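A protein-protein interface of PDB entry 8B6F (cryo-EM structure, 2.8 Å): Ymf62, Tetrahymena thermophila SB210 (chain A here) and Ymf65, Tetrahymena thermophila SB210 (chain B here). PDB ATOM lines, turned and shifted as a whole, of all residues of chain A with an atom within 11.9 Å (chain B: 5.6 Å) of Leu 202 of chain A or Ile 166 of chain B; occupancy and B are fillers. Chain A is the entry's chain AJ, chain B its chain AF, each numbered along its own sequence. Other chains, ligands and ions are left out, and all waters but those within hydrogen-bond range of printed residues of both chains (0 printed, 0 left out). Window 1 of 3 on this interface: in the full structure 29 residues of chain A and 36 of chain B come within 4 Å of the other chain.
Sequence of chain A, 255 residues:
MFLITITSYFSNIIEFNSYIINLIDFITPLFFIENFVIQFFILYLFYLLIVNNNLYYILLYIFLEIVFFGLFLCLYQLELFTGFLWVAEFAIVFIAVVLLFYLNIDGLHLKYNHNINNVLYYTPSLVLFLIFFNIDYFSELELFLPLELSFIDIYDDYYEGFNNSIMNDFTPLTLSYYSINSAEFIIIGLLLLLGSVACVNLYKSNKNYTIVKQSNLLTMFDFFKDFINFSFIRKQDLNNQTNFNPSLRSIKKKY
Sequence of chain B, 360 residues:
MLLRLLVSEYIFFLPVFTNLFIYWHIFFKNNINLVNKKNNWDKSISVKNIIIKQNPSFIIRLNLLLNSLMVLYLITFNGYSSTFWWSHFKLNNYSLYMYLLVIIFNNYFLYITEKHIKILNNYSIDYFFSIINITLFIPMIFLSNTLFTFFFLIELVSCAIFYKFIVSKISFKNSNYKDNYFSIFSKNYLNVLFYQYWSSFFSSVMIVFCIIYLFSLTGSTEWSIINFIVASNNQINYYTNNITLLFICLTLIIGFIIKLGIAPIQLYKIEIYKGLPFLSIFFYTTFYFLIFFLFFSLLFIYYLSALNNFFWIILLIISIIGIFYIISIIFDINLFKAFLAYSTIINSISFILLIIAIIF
O of Ile 166 of chain B is in hydrogen-bond range of OG of Ser 205 of chain A (3.3 Å).
The side-chain hydroxyl (OH) of Tyr 189 of chain B lies close to the side-chain hydroxyl (OG) of Ser 205 of chain A, at 3.4 Å.
The side-chain hydroxyl (OG) of Ser 205 of chain A is in hydrogen-bond range of the backbone carbonyl oxygen (O) of Asn 201 of chain A (3.0 Å).
OH of Tyr 189 of chain B is in hydrogen-bond range of O of Ile 166 of chain B (2.4 Å).
The backbone carbonyl oxygen (O) of Val 197 of chain A lies within hydrogen-bond range of the side-chain amide nitrogen (ND2) of Asn 201 of chain A, 2.5 Å away.
Val 197 of chain A touches Tyr 163 of chain B.
Ala 198 of chain A touches Tyr 163 of chain B (CB to CB, 3.9 Å).
Ala 198 of chain A touches Ile 166 of chain B (O to CD1, 3.8 Å).
Tyr 163 of chain B touches Asn 201 of chain A.
Ile 166 of chain B touches Asn 201 of chain A (CG2 to C, 3.8 Å).
Asn 201 of chain A touches Val 167 of chain B.
Leu 202 of chain A touches Ile 166 of chain B (N to CG2, 3.4 Å).
Tyr 189 of chain B touches Leu 202 of chain A (OH to CD1, 3.7 Å).
Leu 202 of chain A touches Leu 193 of chain B.
Tyr 189 of chain B touches Tyr 209 of chain A.
Of the printed residues of chain B, Leu 202 of chain A touches Ile 166, Tyr 189 and Leu 193.
Printed residues of chain A within 4 Å of Ile 166 of chain B: Ala 198 (3.8 Å), Asn 201 (3.8 Å), Leu 202 (3.4 Å) and Ser 205 (3.3 Å).
No residue of chain A comes within 4 Å of Phe 162 of chain B.
Of the printed residues of chain A, Tyr 163 of chain B touches Leu 194 (3.9 Å), Val 197 (3.5 Å), Ala 198 (3.9 Å) and Asn 201 (3.3 Å).
Of chain A, only Asn 201 (3.6 Å) comes within 4 Å of Val 167 of chain B.
Ser 168 of chain B touches none of the printed residues of chain A.
Printed residues of chain B within 4 Å of Ser 205 of chain A: Ile 166 and Tyr 189.
Printed residues of chain A within 4 Å of Leu 193 of chain B: Leu 202.
Of the printed residues of chain B, Val 197 of chain A touches Tyr 163.
The nearest residue of chain A that does not touch Ile 166 of chain B is Cys 199 of chain A (5.3 Å).
The nearest printed residue of chain B that does not touch Leu 194 of chain A is Ile 161 of chain B (6.0 Å).
Hydrophobic or aromatic side chains of chain A that line the printed part of chain B: Leu 194, Val 197, Ala 198, Leu 202 and Tyr 209.
Along chain A the printed residues that touch a printed residue of chain B span positions 194 to 209.
Hydrophobic or aromatic side chains of chain B that line the printed part of chain A: Tyr 163, Ile 166, Val 167, Tyr 189 and Leu 193.
Among the printed residues, 13 pairs touch across the chains.
Among the printed residues, no Asp or Glu carboxylate lies within 4 Å of a Lys or Arg side-chain nitrogen of the other chain.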
ATOM      1  N   LEU A 191     -17.756  31.296  12.337  1.00  0.00           N
ATOM      2  CA  LEU A 191     -18.093  31.692  13.699  1.00  0.00           C
ATOM      3  C   LEU A 191     -18.631  30.516  14.499  1.00  0.00           C
ATOM      4  O   LEU A 191     -18.273  30.334  15.668  1.00  0.00           O
ATOM      5  CB  LEU A 191     -19.113  32.831  13.660  1.00  0.00           C
ATOM      6  CG  LEU A 191     -19.762  33.247  14.981  1.00  0.00           C
ATOM      7  CD1 LEU A 191     -18.723  33.789  15.934  1.00  0.00           C
ATOM      8  CD2 LEU A 191     -20.849  34.277  14.736  1.00  0.00           C
ATOM      9  N   LEU A 192     -19.498  29.706  13.889  1.00  0.00           N
ATOM     10  CA  LEU A 192     -20.041  28.551  14.594  1.00  0.00           C
ATOM     11  C   LEU A 192     -18.961  27.514  14.876  1.00  0.00           C
ATOM     12  O   LEU A 192     -18.944  26.908  15.953  1.00  0.00           O
ATOM     13  CB  LEU A 192     -21.189  27.944  13.789  1.00  0.00           C
ATOM     14  CG  LEU A 192     -22.416  28.851  13.650  1.00  0.00           C
ATOM     15  CD1 LEU A 192     -23.434  28.243  12.710  1.00  0.00           C
ATOM     16  CD2 LEU A 192     -23.057  29.125  15.001  1.00  0.00           C
ATOM     17  N   LEU A 193     -18.053  27.288  13.923  1.00  0.00           N
ATOM     18  CA  LEU A 193     -16.954  26.359  14.166  1.00  0.00           C
ATOM     19  C   LEU A 193     -16.085  26.839  15.320  1.00  0.00           C
ATOM     20  O   LEU A 193     -15.767  26.074  16.237  1.00  0.00           O
ATOM     21  CB  LEU A 193     -16.117  26.194  12.898  1.00  0.00           C
ATOM     22  CG  LEU A 193     -14.877  25.306  13.031  1.00  0.00           C
ATOM     23  CD1 LEU A 193     -15.256  23.880  13.385  1.00  0.00           C
ATOM     24  CD2 LEU A 193     -14.074  25.342  11.751  1.00  0.00           C
ATOM     25  N   LEU A 194     -15.684  28.110  15.285  1.00  0.00           N
ATOM     26  CA  LEU A 194     -14.862  28.657  16.356  1.00  0.00           C
ATOM     27  C   LEU A 194     -15.609  28.644  17.682  1.00  0.00           C
ATOM     28  O   LEU A 194     -15.000  28.452  18.739  1.00  0.00           O
ATOM     29  CB  LEU A 194     -14.414  30.074  16.005  1.00  0.00           C
ATOM     30  CG  LEU A 194     -13.286  30.656  16.859  1.00  0.00           C
ATOM     31  CD1 LEU A 194     -12.002  29.856  16.713  1.00  0.00           C
ATOM     32  CD2 LEU A 194     -13.051  32.104  16.484  1.00  0.00           C
ATOM     33  N   GLY A 195     -16.926  28.850  17.642  1.00  0.00           N
ATOM     34  CA  GLY A 195     -17.716  28.785  18.860  1.00  0.00           C
ATOM     35  C   GLY A 195     -17.772  27.388  19.444  1.00  0.00           C
ATOM     36  O   GLY A 195     -17.737  27.215  20.665  1.00  0.00           O
ATOM     37  N   SER A 196     -17.861  26.370  18.587  1.00  0.00           N
ATOM     38  CA  SER A 196     -17.785  24.999  19.078  1.00  0.00           C
ATOM     39  C   SER A 196     -16.444  24.739  19.752  1.00  0.00           C
ATOM     40  O   SER A 196     -16.389  24.124  20.824  1.00  0.00           O
ATOM     41  CB  SER A 196     -17.999  24.017  17.928  1.00  0.00           C
ATOM     42  OG  SER A 196     -19.258  24.220  17.311  1.00  0.00           O
ATOM     43  N   VAL A 197     -15.353  25.202  19.143  1.00  0.00           N
ATOM     44  CA  VAL A 197     -14.038  25.032  19.755  1.00  0.00           C
ATOM     45  C   VAL A 197     -13.998  25.734  21.106  1.00  0.00           C
ATOM     46  O   VAL A 197     -13.491  25.186  22.093  1.00  0.00           O
ATOM     47  CB  VAL A 197     -12.938  25.551  18.811  1.00  0.00           C
ATOM     48  CG1 VAL A 197     -11.572  25.495  19.483  1.00  0.00           C
ATOM     49  CG2 VAL A 197     -12.927  24.752  17.519  1.00  0.00           C
ATOM     50  N   ALA A 198     -14.524  26.957  21.171  1.00  0.00           N
ATOM     51  CA  ALA A 198     -14.519  27.701  22.426  1.00  0.00           C
ATOM     52  C   ALA A 198     -15.357  27.001  23.485  1.00  0.00           C
ATOM     53  O   ALA A 198     -14.986  26.972  24.663  1.00  0.00           O
ATOM     54  CB  ALA A 198     -15.031  29.122  22.196  1.00  0.00           C
ATOM     55  N   CYS A 199     -16.498  26.434  23.087  1.00  0.00           N
ATOM     56  CA  CYS A 199     -17.326  25.703  24.039  1.00  0.00           C
ATOM     57  C   CYS A 199     -16.594  24.487  24.591  1.00  0.00           C
ATOM     58  O   CYS A 199     -16.653  24.214  25.795  1.00  0.00           O
ATOM     59  CB  CYS A 199     -18.634  25.279  23.372  1.00  0.00           C
ATOM     60  SG  CYS A 199     -19.798  26.631  23.091  1.00  0.00           S
ATOM     61  N   VAL A 200     -15.898  23.745  23.728  1.00  0.00           N
ATOM     62  CA  VAL A 200     -15.131  22.594  24.194  1.00  0.00           C
ATOM     63  C   VAL A 200     -14.053  23.034  25.175  1.00  0.00           C
ATOM     64  O   VAL A 200     -13.848  22.404  26.219  1.00  0.00           O
ATOM     65  CB  VAL A 200     -14.533  21.836  22.996  1.00  0.00           C
ATOM     66  CG1 VAL A 200     -13.563  20.760  23.461  1.00  0.00           C
ATOM     67  CG2 VAL A 200     -15.637  21.225  22.157  1.00  0.00           C
ATOM     68  N   ASN A 201     -13.343  24.115  24.855  1.00  0.00           N
ATOM     69  CA  ASN A 201     -12.288  24.592  25.743  1.00  0.00           C
ATOM     70  C   ASN A 201     -12.856  25.070  27.072  1.00  0.00           C
ATOM     71  O   ASN A 201     -12.238  24.871  28.125  1.00  0.00           O
ATOM     72  CB  ASN A 201     -11.494  25.698  25.057  1.00  0.00           C
ATOM     73  CG  ASN A 201     -10.578  25.163  23.979  1.00  0.00           C
ATOM     74  OD1 ASN A 201      -9.414  24.864  24.232  1.00  0.00           O
ATOM     75  ND2 ASN A 201     -11.105  25.026  22.769  1.00  0.00           N
ATOM     76  N   LEU A 202     -14.024  25.714  27.046  1.00  0.00           N
ATOM     77  CA  LEU A 202     -14.659  26.136  28.290  1.00  0.00           C
ATOM     78  C   LEU A 202     -15.064  24.935  29.131  1.00  0.00           C
ATOM     79  O   LEU A 202     -14.944  24.961  30.361  1.00  0.00           O
ATOM     80  CB  LEU A 202     -15.866  27.025  27.990  1.00  0.00           C
ATOM     81  CG  LEU A 202     -16.635  27.575  29.196  1.00  0.00           C
ATOM     82  CD1 LEU A 202     -15.708  28.224  30.209  1.00  0.00           C
ATOM     83  CD2 LEU A 202     -17.663  28.578  28.723  1.00  0.00           C
ATOM     84  N   TYR A 203     -15.551  23.875  28.487  1.00  0.00           N
ATOM     85  CA  TYR A 203     -15.861  22.648  29.213  1.00  0.00           C
ATOM     86  C   TYR A 203     -14.616  22.075  29.879  1.00  0.00           C
ATOM     87  O   TYR A 203     -14.662  21.655  31.041  1.00  0.00           O
ATOM     88  CB  TYR A 203     -16.478  21.629  28.257  1.00  0.00           C
ATOM     89  CG  TYR A 203     -16.671  20.256  28.852  1.00  0.00           C
ATOM     90  CD1 TYR A 203     -17.805  19.951  29.591  1.00  0.00           C
ATOM     91  CD2 TYR A 203     -15.724  19.259  28.662  1.00  0.00           C
ATOM     92  CE1 TYR A 203     -17.987  18.696  30.131  1.00  0.00           C
ATOM     93  CE2 TYR A 203     -15.895  18.002  29.197  1.00  0.00           C
ATOM     94  CZ  TYR A 203     -17.028  17.726  29.931  1.00  0.00           C
ATOM     95  OH  TYR A 203     -17.202  16.473  30.466  1.00  0.00           O
ATOM     96  N   LYS A 204     -13.493  22.043  29.159  1.00  0.00           N
ATOM     97  CA  LYS A 204     -12.254  21.545  29.746  1.00  0.00           C
ATOM     98  C   LYS A 204     -11.811  22.419  30.911  1.00  0.00           C
ATOM     99  O   LYS A 204     -11.339  21.911  31.933  1.00  0.00           O
ATOM    100  CB  LYS A 204     -11.158  21.466  28.685  1.00  0.00           C
ATOM    101  CG  LYS A 204     -11.424  20.425  27.608  1.00  0.00           C
ATOM    102  CD  LYS A 204     -10.234  20.252  26.675  1.00  0.00           C
ATOM    103  CE  LYS A 204      -9.973  21.506  25.854  1.00  0.00           C
ATOM    104  NZ  LYS A 204      -8.853  21.318  24.887  1.00  0.00           N
ATOM    105  N   SER A 205     -11.942  23.740  30.770  1.00  0.00           N
ATOM    106  CA  SER A 205     -11.577  24.640  31.858  1.00  0.00           C
ATOM    107  C   SER A 205     -12.444  24.395  33.085  1.00  0.00           C
ATOM    108  O   SER A 205     -11.952  24.417  34.218  1.00  0.00           O
ATOM    109  CB  SER A 205     -11.696  26.093  31.403  1.00  0.00           C
ATOM    110  OG  SER A 205     -10.840  26.352  30.303  1.00  0.00           O
ATOM    111  N   ASN A 206     -13.742  24.172  32.879  1.00  0.00           N
ATOM    112  CA  ASN A 206     -14.616  23.830  33.994  1.00  0.00           C
ATOM    113  C   ASN A 206     -14.175  22.529  34.653  1.00  0.00           C
ATOM    114  O   ASN A 206     -14.192  22.411  35.884  1.00  0.00           O
ATOM    115  CB  ASN A 206     -16.060  23.725  33.503  1.00  0.00           C
ATOM    116  CG  ASN A 206     -17.030  23.387  34.613  1.00  0.00           C
ATOM    117  OD1 ASN A 206     -17.537  24.271  35.300  1.00  0.00           O
ATOM    118  ND2 ASN A 206     -17.303  22.100  34.788  1.00  0.00           N
ATOM    119  N   LYS A 207     -13.777  21.541  33.851  1.00  0.00           N
ATOM    120  CA  LYS A 207     -13.325  20.269  34.404  1.00  0.00           C
ATOM    121  C   LYS A 207     -12.062  20.439  35.237  1.00  0.00           C
ATOM    122  O   LYS A 207     -11.881  19.753  36.248  1.00  0.00           O
ATOM    123  CB  LYS A 207     -13.089  19.261  33.279  1.00  0.00           C
ATOM    124  CG  LYS A 207     -14.291  18.386  32.967  1.00  0.00           C
ATOM    125  CD  LYS A 207     -14.524  17.357  34.062  1.00  0.00           C
ATOM    126  CE  LYS A 207     -15.719  16.472  33.747  1.00  0.00           C
ATOM    127  NZ  LYS A 207     -16.991  17.244  33.689  1.00  0.00           N
ATOM    128  N   ASN A 208     -11.164  21.333  34.824  1.00  0.00           N
ATOM    129  CA  ASN A 208      -9.875  21.445  35.496  1.00  0.00           C
ATOM    130  C   ASN A 208     -10.011  21.730  36.988  1.00  0.00           C
ATOM    131  O   ASN A 208      -9.106  21.384  37.752  1.00  0.00           O
ATOM    132  CB  ASN A 208      -9.026  22.540  34.845  1.00  0.00           C
ATOM    133  CG  ASN A 208      -8.496  22.135  33.482  1.00  0.00           C
ATOM    134  OD1 ASN A 208      -8.226  20.962  33.230  1.00  0.00           O
ATOM    135  ND2 ASN A 208      -8.337  23.112  32.596  1.00  0.00           N
ATOM    136  N   TYR A 209     -11.123  22.324  37.423  1.00  0.00           N
ATOM    137  CA  TYR A 209     -11.273  22.669  38.834  1.00  0.00           C
ATOM    138  C   TYR A 209     -11.210  21.435  39.724  1.00  0.00           C
ATOM    139  O   TYR A 209     -10.568  21.454  40.779  1.00  0.00           O
ATOM    140  CB  TYR A 209     -12.585  23.422  39.056  1.00  0.00           C
ATOM    141  CG  TYR A 209     -12.495  24.890  38.718  1.00  0.00           C
ATOM    142  CD1 TYR A 209     -12.076  25.815  39.666  1.00  0.00           C
ATOM    143  CD2 TYR A 209     -12.825  25.353  37.452  1.00  0.00           C
ATOM    144  CE1 TYR A 209     -11.989  27.157  39.362  1.00  0.00           C
ATOM    145  CE2 TYR A 209     -12.740  26.694  37.139  1.00  0.00           C
ATOM    146  CZ  TYR A 209     -12.321  27.591  38.099  1.00  0.00           C
ATOM    147  OH  TYR A 209     -12.234  28.927  37.795  1.00  0.00           O
ATOM    148  N   THR A 210     -11.874  20.351  39.320  1.00  0.00           N
ATOM    149  CA  THR A 210     -11.809  19.116  40.093  1.00  0.00           C
ATOM    150  C   THR A 210     -10.477  18.396  39.922  1.00  0.00           C
ATOM    151  O   THR A 210     -10.124  17.568  40.765  1.00  0.00           O
ATOM    152  CB  THR A 210     -12.962  18.177  39.718  1.00  0.00           C
ATOM    153  OG1 THR A 210     -12.811  16.930  40.407  1.00  0.00           O
ATOM    154  CG2 THR A 210     -13.012  17.919  38.223  1.00  0.00           C
ATOM    155  N   ILE A 211      -9.730  18.698  38.859  1.00  0.00           N
ATOM    156  CA  ILE A 211      -8.432  18.067  38.644  1.00  0.00           C
ATOM    157  C   ILE A 211      -7.326  18.721  39.463  1.00  0.00           C
ATOM    158  O   ILE A 211      -6.279  18.099  39.678  1.00  0.00           O
ATOM    159  CB  ILE A 211      -8.055  18.109  37.151  1.00  0.00           C
ATOM    160  CG1 ILE A 211      -9.136  17.433  36.303  1.00  0.00           C
ATOM    161  CG2 ILE A 211      -6.703  17.444  36.913  1.00  0.00           C
ATOM    162  CD1 ILE A 211      -8.941  17.599  34.806  1.00  0.00           C
ATOM    163  N   ILE B 161     -11.864  36.368  20.571  1.00  0.00           N
ATOM    164  CA  ILE B 161     -11.344  36.936  21.812  1.00  0.00           C
ATOM    165  C   ILE B 161     -11.964  36.240  23.014  1.00  0.00           C
ATOM    166  O   ILE B 161     -11.302  36.025  24.034  1.00  0.00           O
ATOM    167  CB  ILE B 161     -11.581  38.457  21.843  1.00  0.00           C
ATOM    168  CG1 ILE B 161     -10.746  39.136  20.757  1.00  0.00           C
ATOM    169  CG2 ILE B 161     -11.238  39.027  23.214  1.00  0.00           C
ATOM    170  CD1 ILE B 161     -11.041  40.610  20.577  1.00  0.00           C
ATOM    171  N   PHE B 162     -13.245  35.882  22.917  1.00  0.00           N
ATOM    172  CA  PHE B 162     -13.881  35.124  23.987  1.00  0.00           C
ATOM    173  C   PHE B 162     -13.227  33.758  24.138  1.00  0.00           C
ATOM    174  O   PHE B 162     -13.039  33.267  25.256  1.00  0.00           O
ATOM    175  CB  PHE B 162     -15.377  34.985  23.710  1.00  0.00           C
ATOM    176  CG  PHE B 162     -16.190  34.662  24.929  1.00  0.00           C
ATOM    177  CD1 PHE B 162     -16.260  35.557  25.982  1.00  0.00           C
ATOM    178  CD2 PHE B 162     -16.896  33.476  25.016  1.00  0.00           C
ATOM    179  CE1 PHE B 162     -17.010  35.273  27.102  1.00  0.00           C
ATOM    180  CE2 PHE B 162     -17.649  33.184  26.137  1.00  0.00           C
ATOM    181  CZ  PHE B 162     -17.706  34.084  27.180  1.00  0.00           C
ATOM    182  N   TYR B 163     -12.868  33.133  23.016  1.00  0.00           N
ATOM    183  CA  TYR B 163     -12.106  31.891  23.060  1.00  0.00           C
ATOM    184  C   TYR B 163     -10.780  32.095  23.782  1.00  0.00           C
ATOM    185  O   TYR B 163     -10.395  31.281  24.628  1.00  0.00           O
ATOM    186  CB  TYR B 163     -11.890  31.391  21.628  1.00  0.00           C
ATOM    187  CG  TYR B 163     -11.025  30.159  21.471  1.00  0.00           C
ATOM    188  CD1 TYR B 163     -10.892  29.231  22.492  1.00  0.00           C
ATOM    189  CD2 TYR B 163     -10.345  29.927  20.284  1.00  0.00           C
ATOM    190  CE1 TYR B 163     -10.104  28.108  22.334  1.00  0.00           C
ATOM    191  CE2 TYR B 163      -9.557  28.811  20.118  1.00  0.00           C
ATOM    192  CZ  TYR B 163      -9.439  27.904  21.146  1.00  0.00           C
ATOM    193  OH  TYR B 163      -8.652  26.789  20.983  1.00  0.00           O
ATOM    194  N   LYS B 164     -10.075  33.185  23.469  1.00  0.00           N
ATOM    195  CA  LYS B 164      -8.801  33.468  24.125  1.00  0.00           C
ATOM    196  C   LYS B 164      -8.974  33.634  25.629  1.00  0.00           C
ATOM    197  O   LYS B 164      -8.155  33.144  26.413  1.00  0.00           O
ATOM    198  CB  LYS B 164      -8.166  34.718  23.518  1.00  0.00           C
ATOM    199  CG  LYS B 164      -6.873  35.143  24.201  1.00  0.00           C
ATOM    200  CD  LYS B 164      -6.255  36.357  23.529  1.00  0.00           C
ATOM    201  CE  LYS B 164      -7.101  37.601  23.726  1.00  0.00           C
ATOM    202  NZ  LYS B 164      -6.447  38.810  23.157  1.00  0.00           N
ATOM    203  N   PHE B 165     -10.023  34.342  26.051  1.00  0.00           N
ATOM    204  CA  PHE B 165     -10.285  34.518  27.475  1.00  0.00           C
ATOM    205  C   PHE B 165     -10.692  33.208  28.137  1.00  0.00           C
ATOM    206  O   PHE B 165     -10.374  32.985  29.310  1.00  0.00           O
ATOM    207  CB  PHE B 165     -11.374  35.571  27.690  1.00  0.00           C
ATOM    208  CG  PHE B 165     -10.964  36.972  27.311  1.00  0.00           C
ATOM    209  CD1 PHE B 165      -9.668  37.260  26.908  1.00  0.00           C
ATOM    210  CD2 PHE B 165     -11.883  38.005  27.370  1.00  0.00           C
ATOM    211  CE1 PHE B 165      -9.302  38.547  26.566  1.00  0.00           C
ATOM    212  CE2 PHE B 165     -11.524  39.293  27.028  1.00  0.00           C
ATOM    213  CZ  PHE B 165     -10.233  39.564  26.627  1.00  0.00           C
ATOM    214  N   ILE B 166     -11.398  32.343  27.412  1.00  0.00           N
ATOM    215  CA  ILE B 166     -11.795  31.053  27.968  1.00  0.00           C
ATOM    216  C   ILE B 166     -10.575  30.183  28.248  1.00  0.00           C
ATOM    217  O   ILE B 166     -10.549  29.434  29.230  1.00  0.00           O
ATOM    218  CB  ILE B 166     -12.778  30.356  27.009  1.00  0.00           C
ATOM    219  CG1 ILE B 166     -14.166  30.990  27.115  1.00  0.00           C
ATOM    220  CG2 ILE B 166     -12.847  28.856  27.286  1.00  0.00           C
ATOM    221  CD1 ILE B 166     -15.116  30.566  26.019  1.00  0.00           C
ATOM    222  N   VAL B 167      -9.550  30.266  27.404  1.00  0.00           N
ATOM    223  CA  VAL B 167      -8.411  29.355  27.492  1.00  0.00           C
ATOM    224  C   VAL B 167      -7.325  29.923  28.396  1.00  0.00           C
ATOM    225  O   VAL B 167      -6.179  29.463  28.367  1.00  0.00           O
ATOM    226  CB  VAL B 167      -7.841  29.032  26.098  1.00  0.00           C
ATOM    227  CG1 VAL B 167      -8.846  28.254  25.285  1.00  0.00           C
ATOM    228  CG2 VAL B 167      -7.431  30.296  25.369  1.00  0.00           C
ATOM    229  N   SER B 168      -7.668  30.923  29.201  1.00  0.00           N
ATOM    230  CA  SER B 168      -6.715  31.450  30.167  1.00  0.00           C
ATOM    231  C   SER B 168      -6.407  30.405  31.232  1.00  0.00           C
ATOM    232  O   SER B 168      -7.296  29.694  31.705  1.00  0.00           O
ATOM    233  CB  SER B 168      -7.267  32.715  30.823  1.00  0.00           C
ATOM    234  OG  SER B 168      -7.494  33.729  29.859  1.00  0.00           O
ATOM    235  N   TYR B 189     -12.044  34.508  36.868  1.00  0.00           N
ATOM    236  CA  TYR B 189     -12.417  33.845  35.625  1.00  0.00           C
ATOM    237  C   TYR B 189     -13.869  34.137  35.265  1.00  0.00           C
ATOM    238  O   TYR B 189     -14.171  34.542  34.136  1.00  0.00           O
ATOM    239  CB  TYR B 189     -12.172  32.341  35.760  1.00  0.00           C
ATOM    240  CG  TYR B 189     -12.210  31.567  34.462  1.00  0.00           C
ATOM    241  CD1 TYR B 189     -11.256  31.775  33.476  1.00  0.00           C
ATOM    242  CD2 TYR B 189     -13.172  30.592  34.246  1.00  0.00           C
ATOM    243  CE1 TYR B 189     -11.280  31.056  32.298  1.00  0.00           C
ATOM    244  CE2 TYR B 189     -13.202  29.868  33.073  1.00  0.00           C
ATOM    245  CZ  TYR B 189     -12.252  30.102  32.105  1.00  0.00           C
ATOM    246  OH  TYR B 189     -12.278  29.384  30.934  1.00  0.00           O
ATOM    247  N   LEU B 193     -15.401  36.414  32.044  1.00  0.00           N
ATOM    248  CA  LEU B 193     -16.327  35.829  31.080  1.00  0.00           C
ATOM    249  C   LEU B 193     -17.670  36.547  31.105  1.00  0.00           C
ATOM    250  O   LEU B 193     -18.243  36.849  30.053  1.00  0.00           O
ATOM    251  CB  LEU B 193     -16.510  34.338  31.359  1.00  0.00           C
ATOM    252  CG  LEU B 193     -15.267  33.455  31.206  1.00  0.00           C
ATOM    253  CD1 LEU B 193     -15.624  32.005  31.460  1.00  0.00           C
ATOM    254  CD2 LEU B 193     -14.621  33.611  29.837  1.00  0.00           C
